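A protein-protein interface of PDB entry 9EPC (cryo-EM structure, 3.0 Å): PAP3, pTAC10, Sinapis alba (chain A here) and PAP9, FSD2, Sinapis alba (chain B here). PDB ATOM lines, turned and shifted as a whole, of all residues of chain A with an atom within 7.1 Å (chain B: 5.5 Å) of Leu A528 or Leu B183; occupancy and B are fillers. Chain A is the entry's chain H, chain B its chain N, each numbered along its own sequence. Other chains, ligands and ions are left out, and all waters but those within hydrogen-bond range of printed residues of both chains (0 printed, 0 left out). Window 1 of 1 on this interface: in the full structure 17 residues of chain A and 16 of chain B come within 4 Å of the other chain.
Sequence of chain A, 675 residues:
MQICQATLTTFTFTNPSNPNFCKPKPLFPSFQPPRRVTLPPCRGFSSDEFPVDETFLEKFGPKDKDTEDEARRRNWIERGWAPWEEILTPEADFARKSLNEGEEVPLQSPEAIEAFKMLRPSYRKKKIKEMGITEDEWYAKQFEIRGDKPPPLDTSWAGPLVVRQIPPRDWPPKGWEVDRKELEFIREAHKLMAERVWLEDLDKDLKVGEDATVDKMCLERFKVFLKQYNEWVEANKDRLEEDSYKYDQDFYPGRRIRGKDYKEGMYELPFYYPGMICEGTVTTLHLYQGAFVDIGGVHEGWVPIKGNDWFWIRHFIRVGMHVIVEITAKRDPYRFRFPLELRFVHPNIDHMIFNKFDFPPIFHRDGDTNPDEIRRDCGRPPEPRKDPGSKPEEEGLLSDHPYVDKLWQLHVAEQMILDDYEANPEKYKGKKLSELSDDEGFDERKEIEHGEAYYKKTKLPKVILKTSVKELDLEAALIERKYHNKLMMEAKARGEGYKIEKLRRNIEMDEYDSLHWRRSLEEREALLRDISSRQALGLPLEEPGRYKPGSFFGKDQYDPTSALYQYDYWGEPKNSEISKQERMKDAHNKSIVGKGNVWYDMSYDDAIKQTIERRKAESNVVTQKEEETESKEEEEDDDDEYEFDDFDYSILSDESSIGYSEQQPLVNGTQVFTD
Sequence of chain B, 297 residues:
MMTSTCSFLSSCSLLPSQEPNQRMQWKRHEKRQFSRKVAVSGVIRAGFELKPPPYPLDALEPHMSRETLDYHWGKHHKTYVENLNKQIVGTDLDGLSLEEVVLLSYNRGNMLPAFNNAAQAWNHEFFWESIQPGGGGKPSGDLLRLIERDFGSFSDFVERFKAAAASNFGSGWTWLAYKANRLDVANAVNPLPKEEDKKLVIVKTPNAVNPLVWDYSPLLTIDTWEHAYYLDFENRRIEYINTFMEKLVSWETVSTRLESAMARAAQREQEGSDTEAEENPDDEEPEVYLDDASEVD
The side-chain amide nitrogen of Asn B181 lies within hydrogen-bond range of the side-chain carboxylate of Glu A525 (3.2 Å).
Hydrophobic or aromatic side chains of chain A within 4 Å of the printed part of chain B: Leu A521 and Leu A528. Hydrophobic or aromatic side chains of chain B within 4 Å of the printed part of chain A: Leu B183, Val B185 and Trp B214.
The side-chain amide oxygen (OD1) of Asn B181 sits close to the backbone carbonyl oxygen (O) of Trp B214 (3.4 Å). The backbone carbonyl oxygen (O) of Glu A393 lies within hydrogen-bond range of the guanidinium group (NH1) of Arg A524, 2.6 Å away. The backbone carbonyl oxygen (O) of Arg A529 is in hydrogen-bond range of the side-chain hydroxyl (OG) of Ser A532 (3.5 Å). The side-chain hydroxyl of Ser A533 sits at hydrogen-bond distance from the backbone carbonyl oxygen of Arg A529 (3.1 Å).
Among the printed residues, pairs that only touch across the chains: Ser A532 with Trp B214 (3.0 Å), Leu A528 with Trp B214 (3.0 Å), Glu A394 with Val B185 (3.2 Å), Arg A529 with Trp B214 (3.5 Å), Leu A528 with Leu B183 (3.7 Å), Arg A524 with Leu B183 (3.7 Å) and Leu A521 with Leu B183 (3.9 Å).
Leu A528 touches just these residues of chain B: Leu B183 and Trp B214. Of the printed residues of chain A, Leu B183 touches Leu A521 (3.9 Å), Arg A524 (3.7 Å) and Leu A528 (3.7 Å). Of the printed residues of chain A, Val B185 touches Glu A394. Of the printed residues of chain A, Asn B181 touches Glu A525. Printed residues of chain B within 4 Å of Arg A524: Leu B183. Ser A520 touches none of the printed residues of chain B. Asp B184 touches none of the printed residues of chain A. The nearest printed residue of chain B that does not touch Arg A524 is Val B185 (4.4 Å).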
ATOM      1  N   GLU A 393     -17.627 -26.453 -12.765  1.00  0.00           N
ATOM      2  CA  GLU A 393     -17.810 -25.035 -12.479  1.00  0.00           C
ATOM      3  C   GLU A 393     -19.260 -24.702 -12.156  1.00  0.00           C
ATOM      4  O   GLU A 393     -19.521 -23.756 -11.404  1.00  0.00           O
ATOM      5  CB  GLU A 393     -17.319 -24.192 -13.655  1.00  0.00           C
ATOM      6  CG  GLU A 393     -18.181 -24.270 -14.905  1.00  0.00           C
ATOM      7  CD  GLU A 393     -17.970 -25.547 -15.697  1.00  0.00           C
ATOM      8  OE1 GLU A 393     -17.256 -26.449 -15.210  1.00  0.00           O
ATOM      9  OE2 GLU A 393     -18.517 -25.645 -16.814  1.00  0.00           O
ATOM     10  N   GLU A 394     -20.210 -25.456 -12.700  1.00  0.00           N
ATOM     11  CA  GLU A 394     -21.622 -25.186 -12.475  1.00  0.00           C
ATOM     12  C   GLU A 394     -22.162 -25.858 -11.221  1.00  0.00           C
ATOM     13  O   GLU A 394     -23.342 -25.685 -10.902  1.00  0.00           O
ATOM     14  CB  GLU A 394     -22.447 -25.623 -13.689  1.00  0.00           C
ATOM     15  CG  GLU A 394     -22.508 -27.122 -13.891  1.00  0.00           C
ATOM     16  CD  GLU A 394     -23.207 -27.505 -15.179  1.00  0.00           C
ATOM     17  OE1 GLU A 394     -23.664 -26.596 -15.902  1.00  0.00           O
ATOM     18  OE2 GLU A 394     -23.297 -28.716 -15.470  1.00  0.00           O
ATOM     19  N   LEU A 397     -21.514 -24.041  -4.783  1.00  0.00           N
ATOM     20  CA  LEU A 397     -20.379 -23.820  -3.904  1.00  0.00           C
ATOM     21  C   LEU A 397     -20.592 -24.524  -2.568  1.00  0.00           C
ATOM     22  O   LEU A 397     -21.717 -24.818  -2.159  1.00  0.00           O
ATOM     23  CB  LEU A 397     -20.158 -22.326  -3.682  1.00  0.00           C
ATOM     24  CG  LEU A 397     -19.874 -21.516  -4.945  1.00  0.00           C
ATOM     25  CD1 LEU A 397     -19.575 -20.068  -4.596  1.00  0.00           C
ATOM     26  CD2 LEU A 397     -18.725 -22.135  -5.721  1.00  0.00           C
ATOM     27  N   SER A 520     -14.249 -21.308  -1.374  1.00  0.00           N
ATOM     28  CA  SER A 520     -14.949 -21.914  -2.499  1.00  0.00           C
ATOM     29  C   SER A 520     -15.345 -20.876  -3.540  1.00  0.00           C
ATOM     30  O   SER A 520     -15.500 -21.211  -4.720  1.00  0.00           O
ATOM     31  CB  SER A 520     -16.184 -22.666  -2.008  1.00  0.00           C
ATOM     32  OG  SER A 520     -16.887 -23.248  -3.092  1.00  0.00           O
ATOM     33  N   LEU A 521     -15.506 -19.618  -3.131  1.00  0.00           N
ATOM     34  CA  LEU A 521     -15.928 -18.582  -4.067  1.00  0.00           C
ATOM     35  C   LEU A 521     -14.789 -18.166  -4.987  1.00  0.00           C
ATOM     36  O   LEU A 521     -14.877 -18.319  -6.210  1.00  0.00           O
ATOM     37  CB  LEU A 521     -16.462 -17.369  -3.305  1.00  0.00           C
ATOM     38  CG  LEU A 521     -16.792 -16.173  -4.197  1.00  0.00           C
ATOM     39  CD1 LEU A 521     -17.944 -16.510  -5.125  1.00  0.00           C
ATOM     40  CD2 LEU A 521     -17.106 -14.943  -3.365  1.00  0.00           C
ATOM     41  N   GLU A 522     -13.706 -17.637  -4.413  1.00  0.00           N
ATOM     42  CA  GLU A 522     -12.618 -17.124  -5.238  1.00  0.00           C
ATOM     43  C   GLU A 522     -11.961 -18.229  -6.048  1.00  0.00           C
ATOM     44  O   GLU A 522     -11.381 -17.962  -7.107  1.00  0.00           O
ATOM     45  CB  GLU A 522     -11.586 -16.407  -4.372  1.00  0.00           C
ATOM     46  CG  GLU A 522     -11.076 -17.222  -3.206  1.00  0.00           C
ATOM     47  CD  GLU A 522     -10.383 -16.362  -2.173  1.00  0.00           C
ATOM     48  OE1 GLU A 522      -9.522 -15.543  -2.556  1.00  0.00           O
ATOM     49  OE2 GLU A 522     -10.715 -16.495  -0.977  1.00  0.00           O
ATOM     50  N   GLU A 523     -12.031 -19.471  -5.571  1.00  0.00           N
ATOM     51  CA  GLU A 523     -11.597 -20.589  -6.398  1.00  0.00           C
ATOM     52  C   GLU A 523     -12.494 -20.753  -7.617  1.00  0.00           C
ATOM     53  O   GLU A 523     -12.005 -20.974  -8.730  1.00  0.00           O
ATOM     54  CB  GLU A 523     -11.579 -21.875  -5.578  1.00  0.00           C
ATOM     55  CG  GLU A 523     -11.461 -23.123  -6.423  1.00  0.00           C
ATOM     56  CD  GLU A 523     -11.506 -24.386  -5.602  1.00  0.00           C
ATOM     57  OE1 GLU A 523     -11.100 -24.344  -4.423  1.00  0.00           O
ATOM     58  OE2 GLU A 523     -11.953 -25.420  -6.135  1.00  0.00           O
ATOM     59  N   ARG A 524     -13.811 -20.643  -7.424  1.00  0.00           N
ATOM     60  CA  ARG A 524     -14.743 -20.868  -8.524  1.00  0.00           C
ATOM     61  C   ARG A 524     -14.555 -19.839  -9.629  1.00  0.00           C
ATOM     62  O   ARG A 524     -14.529 -20.184 -10.816  1.00  0.00           O
ATOM     63  CB  ARG A 524     -16.179 -20.844  -8.002  1.00  0.00           C
ATOM     64  CG  ARG A 524     -17.226 -21.081  -9.073  1.00  0.00           C
ATOM     65  CD  ARG A 524     -16.948 -22.363  -9.833  1.00  0.00           C
ATOM     66  NE  ARG A 524     -16.773 -23.498  -8.936  1.00  0.00           N
ATOM     67  CZ  ARG A 524     -17.761 -24.270  -8.507  1.00  0.00           C
ATOM     68  NH1 ARG A 524     -19.013 -24.058  -8.876  1.00  0.00           N
ATOM     69  NH2 ARG A 524     -17.485 -25.279  -7.687  1.00  0.00           N
ATOM     70  N   GLU A 525     -14.427 -18.564  -9.260  1.00  0.00           N
ATOM     71  CA  GLU A 525     -14.208 -17.537 -10.271  1.00  0.00           C
ATOM     72  C   GLU A 525     -12.846 -17.704 -10.932  1.00  0.00           C
ATOM     73  O   GLU A 525     -12.710 -17.500 -12.145  1.00  0.00           O
ATOM     74  CB  GLU A 525     -14.355 -16.148  -9.654  1.00  0.00           C
ATOM     75  CG  GLU A 525     -13.460 -15.898  -8.463  1.00  0.00           C
ATOM     76  CD  GLU A 525     -13.900 -14.701  -7.651  1.00  0.00           C
ATOM     77  OE1 GLU A 525     -15.009 -14.185  -7.907  1.00  0.00           O
ATOM     78  OE2 GLU A 525     -13.140 -14.276  -6.756  1.00  0.00           O
ATOM     79  N   ALA A 526     -11.828 -18.079 -10.156  1.00  0.00           N
ATOM     80  CA  ALA A 526     -10.539 -18.408 -10.752  1.00  0.00           C
ATOM     81  C   ALA A 526     -10.645 -19.636 -11.639  1.00  0.00           C
ATOM     82  O   ALA A 526      -9.964 -19.721 -12.668  1.00  0.00           O
ATOM     83  CB  ALA A 526      -9.490 -18.626  -9.663  1.00  0.00           C
ATOM     84  N   LEU A 527     -11.490 -20.597 -11.258  1.00  0.00           N
ATOM     85  CA  LEU A 527     -11.726 -21.752 -12.114  1.00  0.00           C
ATOM     86  C   LEU A 527     -12.320 -21.331 -13.450  1.00  0.00           C
ATOM     87  O   LEU A 527     -11.924 -21.844 -14.502  1.00  0.00           O
ATOM     88  CB  LEU A 527     -12.644 -22.750 -11.409  1.00  0.00           C
ATOM     89  CG  LEU A 527     -13.173 -23.902 -12.263  1.00  0.00           C
ATOM     90  CD1 LEU A 527     -12.030 -24.727 -12.822  1.00  0.00           C
ATOM     91  CD2 LEU A 527     -14.118 -24.774 -11.452  1.00  0.00           C
ATOM     92  N   LEU A 528     -13.270 -20.394 -13.429  1.00  0.00           N
ATOM     93  CA  LEU A 528     -13.876 -19.930 -14.672  1.00  0.00           C
ATOM     94  C   LEU A 528     -12.834 -19.300 -15.586  1.00  0.00           C
ATOM     95  O   LEU A 528     -12.788 -19.592 -16.786  1.00  0.00           O
ATOM     96  CB  LEU A 528     -15.001 -18.942 -14.371  1.00  0.00           C
ATOM     97  CG  LEU A 528     -16.260 -19.548 -13.755  1.00  0.00           C
ATOM     98  CD1 LEU A 528     -17.321 -18.485 -13.552  1.00  0.00           C
ATOM     99  CD2 LEU A 528     -16.786 -20.667 -14.633  1.00  0.00           C
ATOM    100  N   ARG A 529     -11.974 -18.444 -15.031  1.00  0.00           N
ATOM    101  CA  ARG A 529     -10.928 -17.830 -15.841  1.00  0.00           C
ATOM    102  C   ARG A 529      -9.971 -18.881 -16.384  1.00  0.00           C
ATOM    103  O   ARG A 529      -9.442 -18.739 -17.492  1.00  0.00           O
ATOM    104  CB  ARG A 529     -10.174 -16.778 -15.029  1.00  0.00           C
ATOM    105  CG  ARG A 529     -11.040 -15.614 -14.578  1.00  0.00           C
ATOM    106  CD  ARG A 529     -10.209 -14.466 -14.022  1.00  0.00           C
ATOM    107  NE  ARG A 529      -9.452 -14.845 -12.835  1.00  0.00           N
ATOM    108  CZ  ARG A 529      -8.156 -15.124 -12.832  1.00  0.00           C
ATOM    109  NH1 ARG A 529      -7.435 -15.074 -13.939  1.00  0.00           N
ATOM    110  NH2 ARG A 529      -7.568 -15.458 -11.687  1.00  0.00           N
ATOM    111  N   ASP A 530      -9.741 -19.948 -15.618  1.00  0.00           N
ATOM    112  CA  ASP A 530      -8.894 -21.028 -16.102  1.00  0.00           C
ATOM    113  C   ASP A 530      -9.563 -21.804 -17.229  1.00  0.00           C
ATOM    114  O   ASP A 530      -8.872 -22.344 -18.101  1.00  0.00           O
ATOM    115  CB  ASP A 530      -8.537 -21.968 -14.950  1.00  0.00           C
ATOM    116  CG  ASP A 530      -7.386 -22.892 -15.287  1.00  0.00           C
ATOM    117  OD1 ASP A 530      -6.701 -22.647 -16.302  1.00  0.00           O
ATOM    118  OD2 ASP A 530      -7.164 -23.866 -14.538  1.00  0.00           O
ATOM    119  N   ILE A 531     -10.895 -21.872 -17.231  1.00  0.00           N
ATOM    120  CA  ILE A 531     -11.599 -22.665 -18.236  1.00  0.00           C
ATOM    121  C   ILE A 531     -11.379 -22.085 -19.628  1.00  0.00           C
ATOM    122  O   ILE A 531     -10.987 -22.796 -20.560  1.00  0.00           O
ATOM    123  CB  ILE A 531     -13.096 -22.757 -17.898  1.00  0.00           C
ATOM    124  CG1 ILE A 531     -13.314 -23.657 -16.683  1.00  0.00           C
ATOM    125  CG2 ILE A 531     -13.882 -23.269 -19.092  1.00  0.00           C
ATOM    126  CD1 ILE A 531     -14.757 -23.774 -16.265  1.00  0.00           C
ATOM    127  N   SER A 532     -11.617 -20.782 -19.786  1.00  0.00           N
ATOM    128  CA  SER A 532     -11.511 -20.173 -21.109  1.00  0.00           C
ATOM    129  C   SER A 532     -10.083 -20.215 -21.627  1.00  0.00           C
ATOM    130  O   SER A 532      -9.856 -20.482 -22.813  1.00  0.00           O
ATOM    131  CB  SER A 532     -12.008 -18.734 -21.074  1.00  0.00           C
ATOM    132  OG  SER A 532     -11.043 -17.893 -20.467  1.00  0.00           O
ATOM    133  N   SER A 533      -9.108 -19.946 -20.756  1.00  0.00           N
ATOM    134  CA  SER A 533      -7.714 -19.970 -21.182  1.00  0.00           C
ATOM    135  C   SER A 533      -7.339 -21.337 -21.731  1.00  0.00           C
ATOM    136  O   SER A 533      -6.654 -21.437 -22.755  1.00  0.00           O
ATOM    137  CB  SER A 533      -6.803 -19.586 -20.019  1.00  0.00           C
ATOM    138  OG  SER A 533      -7.105 -18.285 -19.550  1.00  0.00           O
ATOM    139  N   TYR B 106     -20.183 -16.814 -26.119  1.00  0.00           N
ATOM    140  CA  TYR B 106     -19.304 -17.508 -25.185  1.00  0.00           C
ATOM    141  C   TYR B 106     -19.820 -18.911 -24.899  1.00  0.00           C
ATOM    142  O   TYR B 106     -19.047 -19.876 -24.887  1.00  0.00           O
ATOM    143  CB  TYR B 106     -19.181 -16.696 -23.897  1.00  0.00           C
ATOM    144  CG  TYR B 106     -18.312 -17.322 -22.834  1.00  0.00           C
ATOM    145  CD1 TYR B 106     -16.943 -17.440 -23.013  1.00  0.00           C
ATOM    146  CD2 TYR B 106     -18.856 -17.772 -21.641  1.00  0.00           C
ATOM    147  CE1 TYR B 106     -16.143 -18.006 -22.041  1.00  0.00           C
ATOM    148  CE2 TYR B 106     -18.064 -18.336 -20.662  1.00  0.00           C
ATOM    149  CZ  TYR B 106     -16.708 -18.451 -20.869  1.00  0.00           C
ATOM    150  OH  TYR B 106     -15.916 -19.013 -19.897  1.00  0.00           O
ATOM    151  N   ASN B 181     -18.462  -9.543  -9.866  1.00  0.00           N
ATOM    152  CA  ASN B 181     -18.921 -10.855 -10.297  1.00  0.00           C
ATOM    153  C   ASN B 181     -20.208 -11.252  -9.585  1.00  0.00           C
ATOM    154  O   ASN B 181     -20.404 -10.960  -8.402  1.00  0.00           O
ATOM    155  CB  ASN B 181     -17.835 -11.897 -10.033  1.00  0.00           C
ATOM    156  CG  ASN B 181     -18.290 -13.308 -10.342  1.00  0.00           C
ATOM    157  OD1 ASN B 181     -19.172 -13.523 -11.173  1.00  0.00           O
ATOM    158  ND2 ASN B 181     -17.689 -14.281  -9.670  1.00  0.00           N
ATOM    159  N   ARG B 182     -21.089 -11.923 -10.324  1.00  0.00           N
ATOM    160  CA  ARG B 182     -22.299 -12.518  -9.764  1.00  0.00           C
ATOM    161  C   ARG B 182     -22.484 -13.875 -10.422  1.00  0.00           C
ATOM    162  O   ARG B 182     -22.967 -13.958 -11.555  1.00  0.00           O
ATOM    163  CB  ARG B 182     -23.521 -11.628  -9.988  1.00  0.00           C
ATOM    164  CG  ARG B 182     -24.819 -12.230  -9.477  1.00  0.00           C
ATOM    165  CD  ARG B 182     -26.000 -11.310  -9.732  1.00  0.00           C
ATOM    166  NE  ARG B 182     -26.097 -10.930 -11.136  1.00  0.00           N
ATOM    167  CZ  ARG B 182     -26.690 -11.660 -12.071  1.00  0.00           C
ATOM    168  NH1 ARG B 182     -27.251 -12.824 -11.788  1.00  0.00           N
ATOM    169  NH2 ARG B 182     -26.718 -11.211 -13.322  1.00  0.00           N
ATOM    170  N   LEU B 183     -22.093 -14.934  -9.721  1.00  0.00           N
ATOM    171  CA  LEU B 183     -22.177 -16.280 -10.266  1.00  0.00           C
ATOM    172  C   LEU B 183     -23.622 -16.754 -10.316  1.00  0.00           C
ATOM    173  O   LEU B 183     -24.427 -16.443  -9.434  1.00  0.00           O
ATOM    174  CB  LEU B 183     -21.341 -17.245  -9.429  1.00  0.00           C
ATOM    175  CG  LEU B 183     -19.840 -16.961  -9.397  1.00  0.00           C
ATOM    176  CD1 LEU B 183     -19.125 -17.952  -8.497  1.00  0.00           C
ATOM    177  CD2 LEU B 183     -19.269 -17.004 -10.801  1.00  0.00           C
ATOM    178  N   ASP B 184     -23.948 -17.506 -11.364  1.00  0.00           N
ATOM    179  CA  ASP B 184     -25.270 -18.111 -11.503  1.00  0.00           C
ATOM    180  C   ASP B 184     -25.217 -19.561 -11.023  1.00  0.00           C
ATOM    181  O   ASP B 184     -25.394 -20.518 -11.779  1.00  0.00           O
ATOM    182  CB  ASP B 184     -25.748 -18.008 -12.948  1.00  0.00           C
ATOM    183  CG  ASP B 184     -24.716 -18.504 -13.939  1.00  0.00           C
ATOM    184  OD1 ASP B 184     -23.507 -18.378 -13.650  1.00  0.00           O
ATOM    185  OD2 ASP B 184     -25.111 -19.021 -15.005  1.00  0.00           O
ATOM    186  N   VAL B 185     -24.962 -19.707  -9.725  1.00  0.00           N
ATOM    187  CA  VAL B 185     -24.824 -21.007  -9.084  1.00  0.00           C
ATOM    188  C   VAL B 185     -25.322 -20.880  -7.648  1.00  0.00           C
ATOM    189  O   VAL B 185     -25.535 -19.779  -7.138  1.00  0.00           O
ATOM    190  CB  VAL B 185     -23.364 -21.514  -9.125  1.00  0.00           C
ATOM    191  CG1 VAL B 185     -22.549 -20.895  -8.002  1.00  0.00           C
ATOM    192  CG2 VAL B 185     -23.317 -23.029  -9.073  1.00  0.00           C
ATOM    193  N   ALA B 188     -24.073 -18.486  -4.388  1.00  0.00           N
ATOM    194  CA  ALA B 188     -23.206 -17.473  -4.980  1.00  0.00           C
ATOM    195  C   ALA B 188     -23.334 -16.135  -4.267  1.00  0.00           C
ATOM    196  O   ALA B 188     -22.349 -15.397  -4.155  1.00  0.00           O
ATOM    197  CB  ALA B 188     -23.520 -17.313  -6.465  1.00  0.00           C
ATOM    198  N   TRP B 214     -16.639 -13.197 -17.381  1.00  0.00           N
ATOM    199  CA  TRP B 214     -16.654 -13.415 -15.941  1.00  0.00           C
ATOM    200  C   TRP B 214     -17.628 -12.490 -15.234  1.00  0.00           C
ATOM    201  O   TRP B 214     -17.581 -12.384 -14.005  1.00  0.00           O
ATOM    202  CB  TRP B 214     -15.258 -13.224 -15.344  1.00  0.00           C
ATOM    203  CG  TRP B 214     -14.137 -13.616 -16.239  1.00  0.00           C
ATOM    204  CD1 TRP B 214     -13.064 -12.852 -16.589  1.00  0.00           C
ATOM    205  CD2 TRP B 214     -13.973 -14.867 -16.905  1.00  0.00           C
ATOM    206  NE1 TRP B 214     -12.239 -13.552 -17.431  1.00  0.00           N
ATOM    207  CE2 TRP B 214     -12.775 -14.794 -17.640  1.00  0.00           C
ATOM    208  CE3 TRP B 214     -14.721 -16.045 -16.949  1.00  0.00           C
ATOM    209  CZ2 TRP B 214     -12.314 -15.849 -18.412  1.00  0.00           C
ATOM    210  CZ3 TRP B 214     -14.263 -17.089 -17.714  1.00  0.00           C
ATOM    211  CH2 TRP B 214     -13.071 -16.986 -18.434  1.00  0.00           C
